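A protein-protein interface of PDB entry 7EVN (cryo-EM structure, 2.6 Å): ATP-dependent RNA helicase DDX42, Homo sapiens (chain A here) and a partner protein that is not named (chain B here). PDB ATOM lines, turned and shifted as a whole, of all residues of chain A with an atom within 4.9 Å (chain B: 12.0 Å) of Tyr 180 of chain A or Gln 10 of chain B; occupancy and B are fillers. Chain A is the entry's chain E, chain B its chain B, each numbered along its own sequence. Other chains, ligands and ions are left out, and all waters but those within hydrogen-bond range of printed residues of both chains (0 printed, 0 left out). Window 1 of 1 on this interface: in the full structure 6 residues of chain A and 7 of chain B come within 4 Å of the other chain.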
ATOM      1  N   ASP A 176      -6.099 -21.691   1.882  1.00  0.00           N
ATOM      2  CA  ASP A 176      -4.717 -22.231   1.998  1.00  0.00           C
ATOM      3  C   ASP A 176      -4.271 -22.784   0.640  1.00  0.00           C
ATOM      4  O   ASP A 176      -3.137 -22.474   0.225  1.00  0.00           O
ATOM      5  CB  ASP A 176      -4.637 -23.325   3.064  1.00  0.00           C
ATOM      6  CG  ASP A 176      -4.348 -22.797   4.457  1.00  0.00           C
ATOM      7  OD1 ASP A 176      -4.088 -21.585   4.579  1.00  0.00           O
ATOM      8  OD2 ASP A 176      -4.379 -23.605   5.408  1.00  0.00           O
ATOM      9  N   GLN A 177      -5.149 -23.521  -0.046  1.00  0.00           N
ATOM     10  CA  GLN A 177      -4.803 -24.108  -1.367  1.00  0.00           C
ATOM     11  C   GLN A 177      -4.526 -22.985  -2.371  1.00  0.00           C
ATOM     12  O   GLN A 177      -3.525 -23.088  -3.109  1.00  0.00           O
ATOM     13  CB  GLN A 177      -5.925 -25.022  -1.856  1.00  0.00           C
ATOM     14  CG  GLN A 177      -5.928 -26.389  -1.189  1.00  0.00           C
ATOM     15  CD  GLN A 177      -6.931 -27.317  -1.822  1.00  0.00           C
ATOM     16  OE1 GLN A 177      -7.606 -26.965  -2.787  1.00  0.00           O
ATOM     17  NE2 GLN A 177      -7.037 -28.520  -1.281  1.00  0.00           N
ATOM     18  N   GLU A 178      -5.349 -21.934  -2.361  1.00  0.00           N
ATOM     19  CA  GLU A 178      -5.146 -20.807  -3.309  1.00  0.00           C
ATOM     20  C   GLU A 178      -3.788 -20.165  -3.022  1.00  0.00           C
ATOM     21  O   GLU A 178      -3.039 -19.909  -3.983  1.00  0.00           O
ATOM     22  CB  GLU A 178      -6.243 -19.756  -3.135  1.00  0.00           C
ATOM     23  CG  GLU A 178      -7.593 -20.183  -3.678  1.00  0.00           C
ATOM     24  CD  GLU A 178      -8.555 -19.030  -3.903  1.00  0.00           C
ATOM     25  OE1 GLU A 178      -8.101 -17.871  -3.879  1.00  0.00           O
ATOM     26  OE2 GLU A 178      -9.756 -19.294  -4.106  1.00  0.00           O
ATOM     27  N   ALA A 179      -3.463 -19.981  -1.740  1.00  0.00           N
ATOM     28  CA  ALA A 179      -2.183 -19.351  -1.353  1.00  0.00           C
ATOM     29  C   ALA A 179      -1.029 -20.221  -1.853  1.00  0.00           C
ATOM     30  O   ALA A 179      -0.089 -19.664  -2.441  1.00  0.00           O
ATOM     31  CB  ALA A 179      -2.136 -19.185   0.145  1.00  0.00           C
ATOM     32  N   TYR A 180      -1.142 -21.542  -1.692  1.00  0.00           N
ATOM     33  CA  TYR A 180      -0.063 -22.460  -2.142  1.00  0.00           C
ATOM     34  C   TYR A 180       0.107 -22.359  -3.663  1.00  0.00           C
ATOM     35  O   TYR A 180       1.258 -22.228  -4.134  1.00  0.00           O
ATOM     36  CB  TYR A 180      -0.372 -23.895  -1.709  1.00  0.00           C
ATOM     37  CG  TYR A 180       0.552 -24.933  -2.290  1.00  0.00           C
ATOM     38  CD1 TYR A 180       0.069 -25.944  -3.101  1.00  0.00           C
ATOM     39  CD2 TYR A 180       1.913 -24.894  -2.044  1.00  0.00           C
ATOM     40  CE1 TYR A 180       0.914 -26.898  -3.646  1.00  0.00           C
ATOM     41  CE2 TYR A 180       2.771 -25.838  -2.581  1.00  0.00           C
ATOM     42  CZ  TYR A 180       2.270 -26.844  -3.385  1.00  0.00           C
ATOM     43  OH  TYR A 180       3.108 -27.781  -3.916  1.00  0.00           O
ATOM     44  N   PHE A 181      -1.004 -22.340  -4.405  1.00  0.00           N
ATOM     45  CA  PHE A 181      -0.902 -22.256  -5.886  1.00  0.00           C
ATOM     46  C   PHE A 181      -0.236 -20.933  -6.271  1.00  0.00           C
ATOM     47  O   PHE A 181       0.657 -20.937  -7.142  1.00  0.00           O
ATOM     48  CB  PHE A 181      -2.281 -22.389  -6.539  1.00  0.00           C
ATOM     49  CG  PHE A 181      -2.991 -23.693  -6.275  1.00  0.00           C
ATOM     50  CD1 PHE A 181      -2.285 -24.880  -6.175  1.00  0.00           C
ATOM     51  CD2 PHE A 181      -4.369 -23.735  -6.148  1.00  0.00           C
ATOM     52  CE1 PHE A 181      -2.939 -26.077  -5.935  1.00  0.00           C
ATOM     53  CE2 PHE A 181      -5.024 -24.934  -5.911  1.00  0.00           C
ATOM     54  CZ  PHE A 181      -4.307 -26.101  -5.804  1.00  0.00           C
ATOM     55  N   ARG A 182      -0.618 -19.848  -5.590  1.00  0.00           N
ATOM     56  CA  ARG A 182      -0.060 -18.503  -5.879  1.00  0.00           C
ATOM     57  C   ARG A 182       1.446 -18.513  -5.615  1.00  0.00           C
ATOM     58  O   ARG A 182       2.197 -18.007  -6.466  1.00  0.00           O
ATOM     59  CB  ARG A 182      -0.737 -17.470  -4.975  1.00  0.00           C
ATOM     60  CG  ARG A 182      -1.863 -16.693  -5.642  1.00  0.00           C
ATOM     61  CD  ARG A 182      -1.489 -15.233  -5.805  1.00  0.00           C
ATOM     62  NE  ARG A 182      -1.512 -14.535  -4.527  1.00  0.00           N
ATOM     63  CZ  ARG A 182      -0.549 -14.599  -3.614  1.00  0.00           C
ATOM     64  NH1 ARG A 182       0.527 -15.334  -3.837  1.00  0.00           N
ATOM     65  NH2 ARG A 182      -0.663 -13.929  -2.483  1.00  0.00           N
ATOM     66  N   TYR A 183       1.869 -19.126  -4.506  1.00  0.00           N
ATOM     67  CA  TYR A 183       3.310 -19.181  -4.153  1.00  0.00           C
ATOM     68  C   TYR A 183       4.059 -19.957  -5.238  1.00  0.00           C
ATOM     69  O   TYR A 183       5.111 -19.479  -5.710  1.00  0.00           O
ATOM     70  CB  TYR A 183       3.482 -19.851  -2.788  1.00  0.00           C
ATOM     71  CG  TYR A 183       4.910 -20.116  -2.384  1.00  0.00           C
ATOM     72  CD1 TYR A 183       5.510 -21.336  -2.644  1.00  0.00           C
ATOM     73  CD2 TYR A 183       5.658 -19.151  -1.734  1.00  0.00           C
ATOM     74  CE1 TYR A 183       6.820 -21.589  -2.271  1.00  0.00           C
ATOM     75  CE2 TYR A 183       6.967 -19.387  -1.353  1.00  0.00           C
ATOM     76  CZ  TYR A 183       7.552 -20.610  -1.624  1.00  0.00           C
ATOM     77  OH  TYR A 183       8.842 -20.852  -1.253  1.00  0.00           O
ATOM     78  N   MET A 184       3.488 -21.080  -5.680  1.00  0.00           N
ATOM     79  CA  MET A 184       4.170 -21.885  -6.726  1.00  0.00           C
ATOM     80  C   MET A 184       4.290 -21.054  -8.008  1.00  0.00           C
ATOM     81  O   MET A 184       5.388 -21.031  -8.590  1.00  0.00           O
ATOM     82  CB  MET A 184       3.387 -23.168  -7.021  1.00  0.00           C
ATOM     83  CG  MET A 184       3.367 -24.129  -5.854  1.00  0.00           C
ATOM     84  SD  MET A 184       5.019 -24.362  -5.155  1.00  0.00           S
ATOM     85  CE  MET A 184       5.833 -25.212  -6.504  1.00  0.00           C
ATOM     86  N   ARG B   4       5.303 -29.566 -10.618  1.00  0.00           N
ATOM     87  CA  ARG B   4       6.093 -28.992  -9.535  1.00  0.00           C
ATOM     88  C   ARG B   4       5.366 -29.090  -8.195  1.00  0.00           C
ATOM     89  O   ARG B   4       5.940 -28.807  -7.147  1.00  0.00           O
ATOM     90  CB  ARG B   4       6.433 -27.531  -9.843  1.00  0.00           C
ATOM     91  CG  ARG B   4       7.417 -27.359 -10.983  1.00  0.00           C
ATOM     92  CD  ARG B   4       7.908 -25.923 -11.091  1.00  0.00           C
ATOM     93  NE  ARG B   4       8.383 -25.390  -9.818  1.00  0.00           N
ATOM     94  CZ  ARG B   4       9.582 -25.639  -9.304  1.00  0.00           C
ATOM     95  NH1 ARG B   4      10.435 -26.422  -9.950  1.00  0.00           N
ATOM     96  NH2 ARG B   4       9.932 -25.108  -8.140  1.00  0.00           N
ATOM     97  N   TYR B   5       4.097 -29.497  -8.245  1.00  0.00           N
ATOM     98  CA  TYR B   5       3.234 -29.604  -7.073  1.00  0.00           C
ATOM     99  C   TYR B   5       3.461 -30.903  -6.307  1.00  0.00           C
ATOM    100  O   TYR B   5       2.906 -31.941  -6.668  1.00  0.00           O
ATOM    101  CB  TYR B   5       1.767 -29.511  -7.482  1.00  0.00           C
ATOM    102  CG  TYR B   5       1.329 -28.191  -8.063  1.00  0.00           C
ATOM    103  CD1 TYR B   5       0.434 -28.153  -9.115  1.00  0.00           C
ATOM    104  CD2 TYR B   5       1.786 -26.988  -7.550  1.00  0.00           C
ATOM    105  CE1 TYR B   5       0.016 -26.965  -9.652  1.00  0.00           C
ATOM    106  CE2 TYR B   5       1.366 -25.785  -8.083  1.00  0.00           C
ATOM    107  CZ  TYR B   5       0.481 -25.784  -9.135  1.00  0.00           C
ATOM    108  OH  TYR B   5       0.055 -24.599  -9.685  1.00  0.00           O
ATOM    109  N   THR B   6       4.282 -30.877  -5.264  1.00  0.00           N
ATOM    110  CA  THR B   6       4.458 -32.074  -4.457  1.00  0.00           C
ATOM    111  C   THR B   6       3.880 -31.882  -3.060  1.00  0.00           C
ATOM    112  O   THR B   6       3.543 -30.771  -2.647  1.00  0.00           O
ATOM    113  CB  THR B   6       5.936 -32.451  -4.360  1.00  0.00           C
ATOM    114  OG1 THR B   6       6.721 -31.277  -4.129  1.00  0.00           O
ATOM    115  CG2 THR B   6       6.395 -33.113  -5.646  1.00  0.00           C
ATOM    116  N   ILE B   7       3.752 -32.995  -2.336  1.00  0.00           N
ATOM    117  CA  ILE B   7       3.365 -32.962  -0.934  1.00  0.00           C
ATOM    118  C   ILE B   7       4.416 -32.285  -0.069  1.00  0.00           C
ATOM    119  O   ILE B   7       4.067 -31.561   0.866  1.00  0.00           O
ATOM    120  CB  ILE B   7       3.075 -34.401  -0.441  1.00  0.00           C
ATOM    121  CG1 ILE B   7       1.597 -34.738  -0.600  1.00  0.00           C
ATOM    122  CG2 ILE B   7       3.483 -34.593   1.005  1.00  0.00           C
ATOM    123  CD1 ILE B   7       1.251 -36.148  -0.209  1.00  0.00           C
ATOM    124  N   HIS B   8       5.699 -32.478  -0.381  1.00  0.00           N
ATOM    125  CA  HIS B   8       6.771 -31.931   0.442  1.00  0.00           C
ATOM    126  C   HIS B   8       6.823 -30.409   0.373  1.00  0.00           C
ATOM    127  O   HIS B   8       7.046 -29.750   1.392  1.00  0.00           O
ATOM    128  CB  HIS B   8       8.112 -32.529   0.018  1.00  0.00           C
ATOM    129  CG  HIS B   8       9.295 -31.711   0.428  1.00  0.00           C
ATOM    130  ND1 HIS B   8       9.940 -31.887   1.632  1.00  0.00           N
ATOM    131  CD2 HIS B   8       9.949 -30.709  -0.205  1.00  0.00           C
ATOM    132  CE1 HIS B   8      10.938 -31.028   1.725  1.00  0.00           C
ATOM    133  NE2 HIS B   8      10.965 -30.301   0.623  1.00  0.00           N
ATOM    134  N   SER B   9       6.641 -29.830  -0.812  1.00  0.00           N
ATOM    135  CA  SER B   9       6.611 -28.380  -0.912  1.00  0.00           C
ATOM    136  C   SER B   9       5.295 -27.796  -0.424  1.00  0.00           C
ATOM    137  O   SER B   9       5.220 -26.588  -0.185  1.00  0.00           O
ATOM    138  CB  SER B   9       6.872 -27.930  -2.351  1.00  0.00           C
ATOM    139  OG  SER B   9       6.317 -28.837  -3.280  1.00  0.00           O
ATOM    140  N   GLN B  10       4.256 -28.619  -0.284  1.00  0.00           N
ATOM    141  CA  GLN B  10       3.024 -28.149   0.332  1.00  0.00           C
ATOM    142  C   GLN B  10       3.153 -28.133   1.846  1.00  0.00           C
ATOM    143  O   GLN B  10       2.601 -27.256   2.515  1.00  0.00           O
ATOM    144  CB  GLN B  10       1.851 -29.025  -0.101  1.00  0.00           C
ATOM    145  CG  GLN B  10       0.489 -28.411   0.162  1.00  0.00           C
ATOM    146  CD  GLN B  10      -0.551 -29.440   0.544  1.00  0.00           C
ATOM    147  OE1 GLN B  10      -0.246 -30.620   0.686  1.00  0.00           O
ATOM    148  NE2 GLN B  10      -1.780 -28.996   0.729  1.00  0.00           N
ATOM    149  N   LEU B  11       3.887 -29.097   2.399  1.00  0.00           N
ATOM    150  CA  LEU B  11       4.135 -29.109   3.833  1.00  0.00           C
ATOM    151  C   LEU B  11       4.979 -27.915   4.255  1.00  0.00           C
ATOM    152  O   LEU B  11       4.660 -27.239   5.237  1.00  0.00           O
ATOM    153  CB  LEU B  11       4.819 -30.415   4.230  1.00  0.00           C
ATOM    154  CG  LEU B  11       5.492 -30.442   5.597  1.00  0.00           C
ATOM    155  CD1 LEU B  11       4.456 -30.429   6.695  1.00  0.00           C
ATOM    156  CD2 LEU B  11       6.386 -31.654   5.725  1.00  0.00           C
ATOM    157  N   GLU B  12       6.056 -27.636   3.522  1.00  0.00           N
ATOM    158  CA  GLU B  12       6.933 -26.531   3.880  1.00  0.00           C
ATOM    159  C   GLU B  12       6.249 -25.179   3.754  1.00  0.00           C
ATOM    160  O   GLU B  12       6.557 -24.273   4.531  1.00  0.00           O
ATOM    161  CB  GLU B  12       8.188 -26.562   3.015  1.00  0.00           C
ATOM    162  CG  GLU B  12       9.236 -27.520   3.526  1.00  0.00           C
ATOM    163  CD  GLU B  12      10.612 -26.901   3.596  1.00  0.00           C
ATOM    164  OE1 GLU B  12      10.784 -25.917   4.343  1.00  0.00           O
ATOM    165  OE2 GLU B  12      11.526 -27.406   2.911  1.00  0.00           O
ATOM    166  N   HIS B  13       5.337 -25.020   2.796  1.00  0.00           N
ATOM    167  CA  HIS B  13       4.600 -23.771   2.677  1.00  0.00           C
ATOM    168  C   HIS B  13       3.567 -23.607   3.786  1.00  0.00           C
ATOM    169  O   HIS B  13       3.317 -22.483   4.228  1.00  0.00           O
ATOM    170  CB  HIS B  13       3.929 -23.693   1.308  1.00  0.00           C
ATOM    171  CG  HIS B  13       2.929 -22.587   1.185  1.00  0.00           C
ATOM    172  ND1 HIS B  13       1.594 -22.756   1.479  1.00  0.00           N
ATOM    173  CD2 HIS B  13       3.067 -21.296   0.801  1.00  0.00           C
ATOM    174  CE1 HIS B  13       0.954 -21.620   1.283  1.00  0.00           C
ATOM    175  NE2 HIS B  13       1.824 -20.717   0.869  1.00  0.00           N
ATOM    176  N   LEU B  14       2.969 -24.705   4.255  1.00  0.00           N
ATOM    177  CA  LEU B  14       2.038 -24.621   5.374  1.00  0.00           C
ATOM    178  C   LEU B  14       2.755 -24.403   6.698  1.00  0.00           C
ATOM    179  O   LEU B  14       2.154 -23.881   7.640  1.00  0.00           O
ATOM    180  CB  LEU B  14       1.177 -25.882   5.454  1.00  0.00           C
ATOM    181  CG  LEU B  14       0.106 -26.103   4.383  1.00  0.00           C
ATOM    182  CD1 LEU B  14      -0.540 -27.465   4.553  1.00  0.00           C
ATOM    183  CD2 LEU B  14      -0.941 -25.003   4.400  1.00  0.00           C
ATOM    184  N   GLN B  15       4.023 -24.803   6.798  1.00  0.00           N
ATOM    185  CA  GLN B  15       4.796 -24.488   7.992  1.00  0.00           C
ATOM    186  C   GLN B  15       5.057 -22.993   8.102  1.00  0.00           C
ATOM    187  O   GLN B  15       4.974 -22.430   9.198  1.00  0.00           O
ATOM    188  CB  GLN B  15       6.114 -25.257   7.987  1.00  0.00           C
ATOM    189  CG  GLN B  15       5.973 -26.727   8.333  1.00  0.00           C
ATOM    190  CD  GLN B  15       7.170 -27.265   9.083  1.00  0.00           C
ATOM    191  OE1 GLN B  15       7.085 -28.283   9.764  1.00  0.00           O
ATOM    192  NE2 GLN B  15       8.298 -26.586   8.957  1.00  0.00           N
ATOM    193  N   SER B  16       5.349 -22.331   6.986  1.00  0.00           N
ATOM    194  CA  SER B  16       5.594 -20.898   6.967  1.00  0.00           C
ATOM    195  C   SER B  16       4.350 -20.079   7.267  1.00  0.00           C
ATOM    196  O   SER B  16       4.459 -18.872   7.490  1.00  0.00           O
ATOM    197  CB  SER B  16       6.165 -20.478   5.611  1.00  0.00           C
ATOM    198  OG  SER B  16       5.173 -20.498   4.604  1.00  0.00           O
ATOM    199  N   LYS B  17       3.177 -20.701   7.274  1.00  0.00           N
ATOM    200  CA  LYS B  17       1.928 -20.025   7.582  1.00  0.00           C
ATOM    201  C   LYS B  17       1.593 -20.059   9.064  1.00  0.00           C
ATOM    202  O   LYS B  17       0.784 -19.250   9.521  1.00  0.00           O
ATOM    203  CB  LYS B  17       0.784 -20.650   6.780  1.00  0.00           C
ATOM    204  CG  LYS B  17       0.159 -19.729   5.755  1.00  0.00           C
ATOM    205  CD  LYS B  17       1.181 -19.253   4.752  1.00  0.00           C
ATOM    206  CE  LYS B  17       0.538 -18.369   3.706  1.00  0.00           C
ATOM    207  NZ  LYS B  17      -0.171 -17.219   4.330  1.00  0.00           N
ATOM    208  N   TYR B  18       2.191 -20.976   9.817  1.00  0.00           N
ATOM    209  CA  TYR B  18       1.992 -21.072  11.255  1.00  0.00           C
ATOM    210  C   TYR B  18       2.722 -19.920  11.938  1.00  0.00           C
ATOM    211  O   TYR B  18       3.943 -19.794  11.815  1.00  0.00           O
ATOM    212  CB  TYR B  18       2.497 -22.420  11.765  1.00  0.00           C
ATOM    213  CG  TYR B  18       1.944 -22.819  13.107  1.00  0.00           C
ATOM    214  CD1 TYR B  18       0.861 -23.679  13.206  1.00  0.00           C
ATOM    215  CD2 TYR B  18       2.503 -22.333  14.277  1.00  0.00           C
ATOM    216  CE1 TYR B  18       0.351 -24.041  14.439  1.00  0.00           C
ATOM    217  CE2 TYR B  18       2.002 -22.685  15.506  1.00  0.00           C
ATOM    218  CZ  TYR B  18       0.928 -23.535  15.586  1.00  0.00           C
ATOM    219  OH  TYR B  18       0.441 -23.880  16.823  1.00  0.00           O
ATOM    220  N   THR B  21       6.765 -19.044  13.259  1.00  0.00           N
ATOM    221  CA  THR B  21       7.764 -19.745  12.466  1.00  0.00           C
ATOM    222  C   THR B  21       8.642 -18.730  11.737  1.00  0.00           C
ATOM    223  O   THR B  21       8.189 -17.629  11.410  1.00  0.00           O
ATOM    224  CB  THR B  21       7.044 -20.685  11.489  1.00  0.00           C
ATOM    225  OG1 THR B  21       7.164 -22.040  11.931  1.00  0.00           O
ATOM    226  CG2 THR B  21       7.556 -20.549  10.073  1.00  0.00           C
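O of Thr 6 of chain B sits at hydrogen-bond distance from OH of Tyr 180 of chain A, at 3.3 Å.
The side-chain hydroxyl (OH) of Tyr 180 of chain A lies within hydrogen-bond range of the side-chain hydroxyl (OG) of Ser 9 of chain B (3.4 Å).
The backbone carbonyl oxygen of His 13 of chain B sits at hydrogen-bond distance from the side-chain hydroxyl of Ser 16 of chain B.
OG1 of Thr 6 of chain B is in hydrogen-bond range of OG of Ser 9 of chain B, 2.6 Å away.
Asp 176 of chain A touches one residue of chain B.
No residue of chain B comes within 4 Å of Gln 177 of chain A.
Of chain B, only Tyr 5, Thr 6, Ser 9, Gln 10 and His 13 come within 4 Å of Tyr 180 of chain A.
Phe 181 of chain A touches none of the printed residues of chain B.
Arg 182 of chain A touches none of the printed residues of chain B.
Printed residues of chain B within 4 Å of Tyr 183 of chain A: His 13 (3.9 Å).
Met 184 of chain A touches just these residues of chain B: Arg 4 and Tyr 5.
Of the printed residues of chain A, Ser 9 of chain B touches Tyr 180.
Of chain A, only Tyr 180 comes within 4 Å of Gln 10 of chain B.
Of the printed residues of chain A, His 13 of chain B touches Ala 179, Tyr 180 and Tyr 183.
The nearest printed residue of chain A that does not touch Gln 10 of chain B is Gln 177 of chain A (5.3 Å).
The nearest printed residue of chain A that does not touch Thr 6 of chain B is Met 184 of chain A (6.0 Å).
Of the 9 printed residues of chain A, 5 touch a printed residue of chain B.
Hydrophobic or aromatic side chains of chain A within 4 Å of the printed part of chain B: Tyr 180, Tyr 183 and Met 184.
Among the printed residues, no Asp or Glu carboxylate lies within 4 Å of a Lys or Arg side-chain nitrogen of the other chain.
Leu 14 of chain B touches Asp 176 of chain A (CD2 to OD2, 3.8 Å).
His 13 of chain B touches Ala 179 of chain A (CE1 to C, 3.97 Å).
Tyr 180 of chain A touches Tyr 5 of chain B (OH to CA, 3.6 Å).
CA of Gln 10 of chain B touches CE2 of Tyr 180 of chain A, at 3.7 Å.
His 13 of chain B touches Tyr 180 of chain A (CE1 to N, 3.6 Å).
Tyr 183 of chain A touches His 13 of chain B (CG to CD2, 3.9 Å).
O of Arg 4 of chain B touches CE of Met 184 of chain A, 3.7 Å away.
Met 184 of chain A touches Tyr 5 of chain B.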
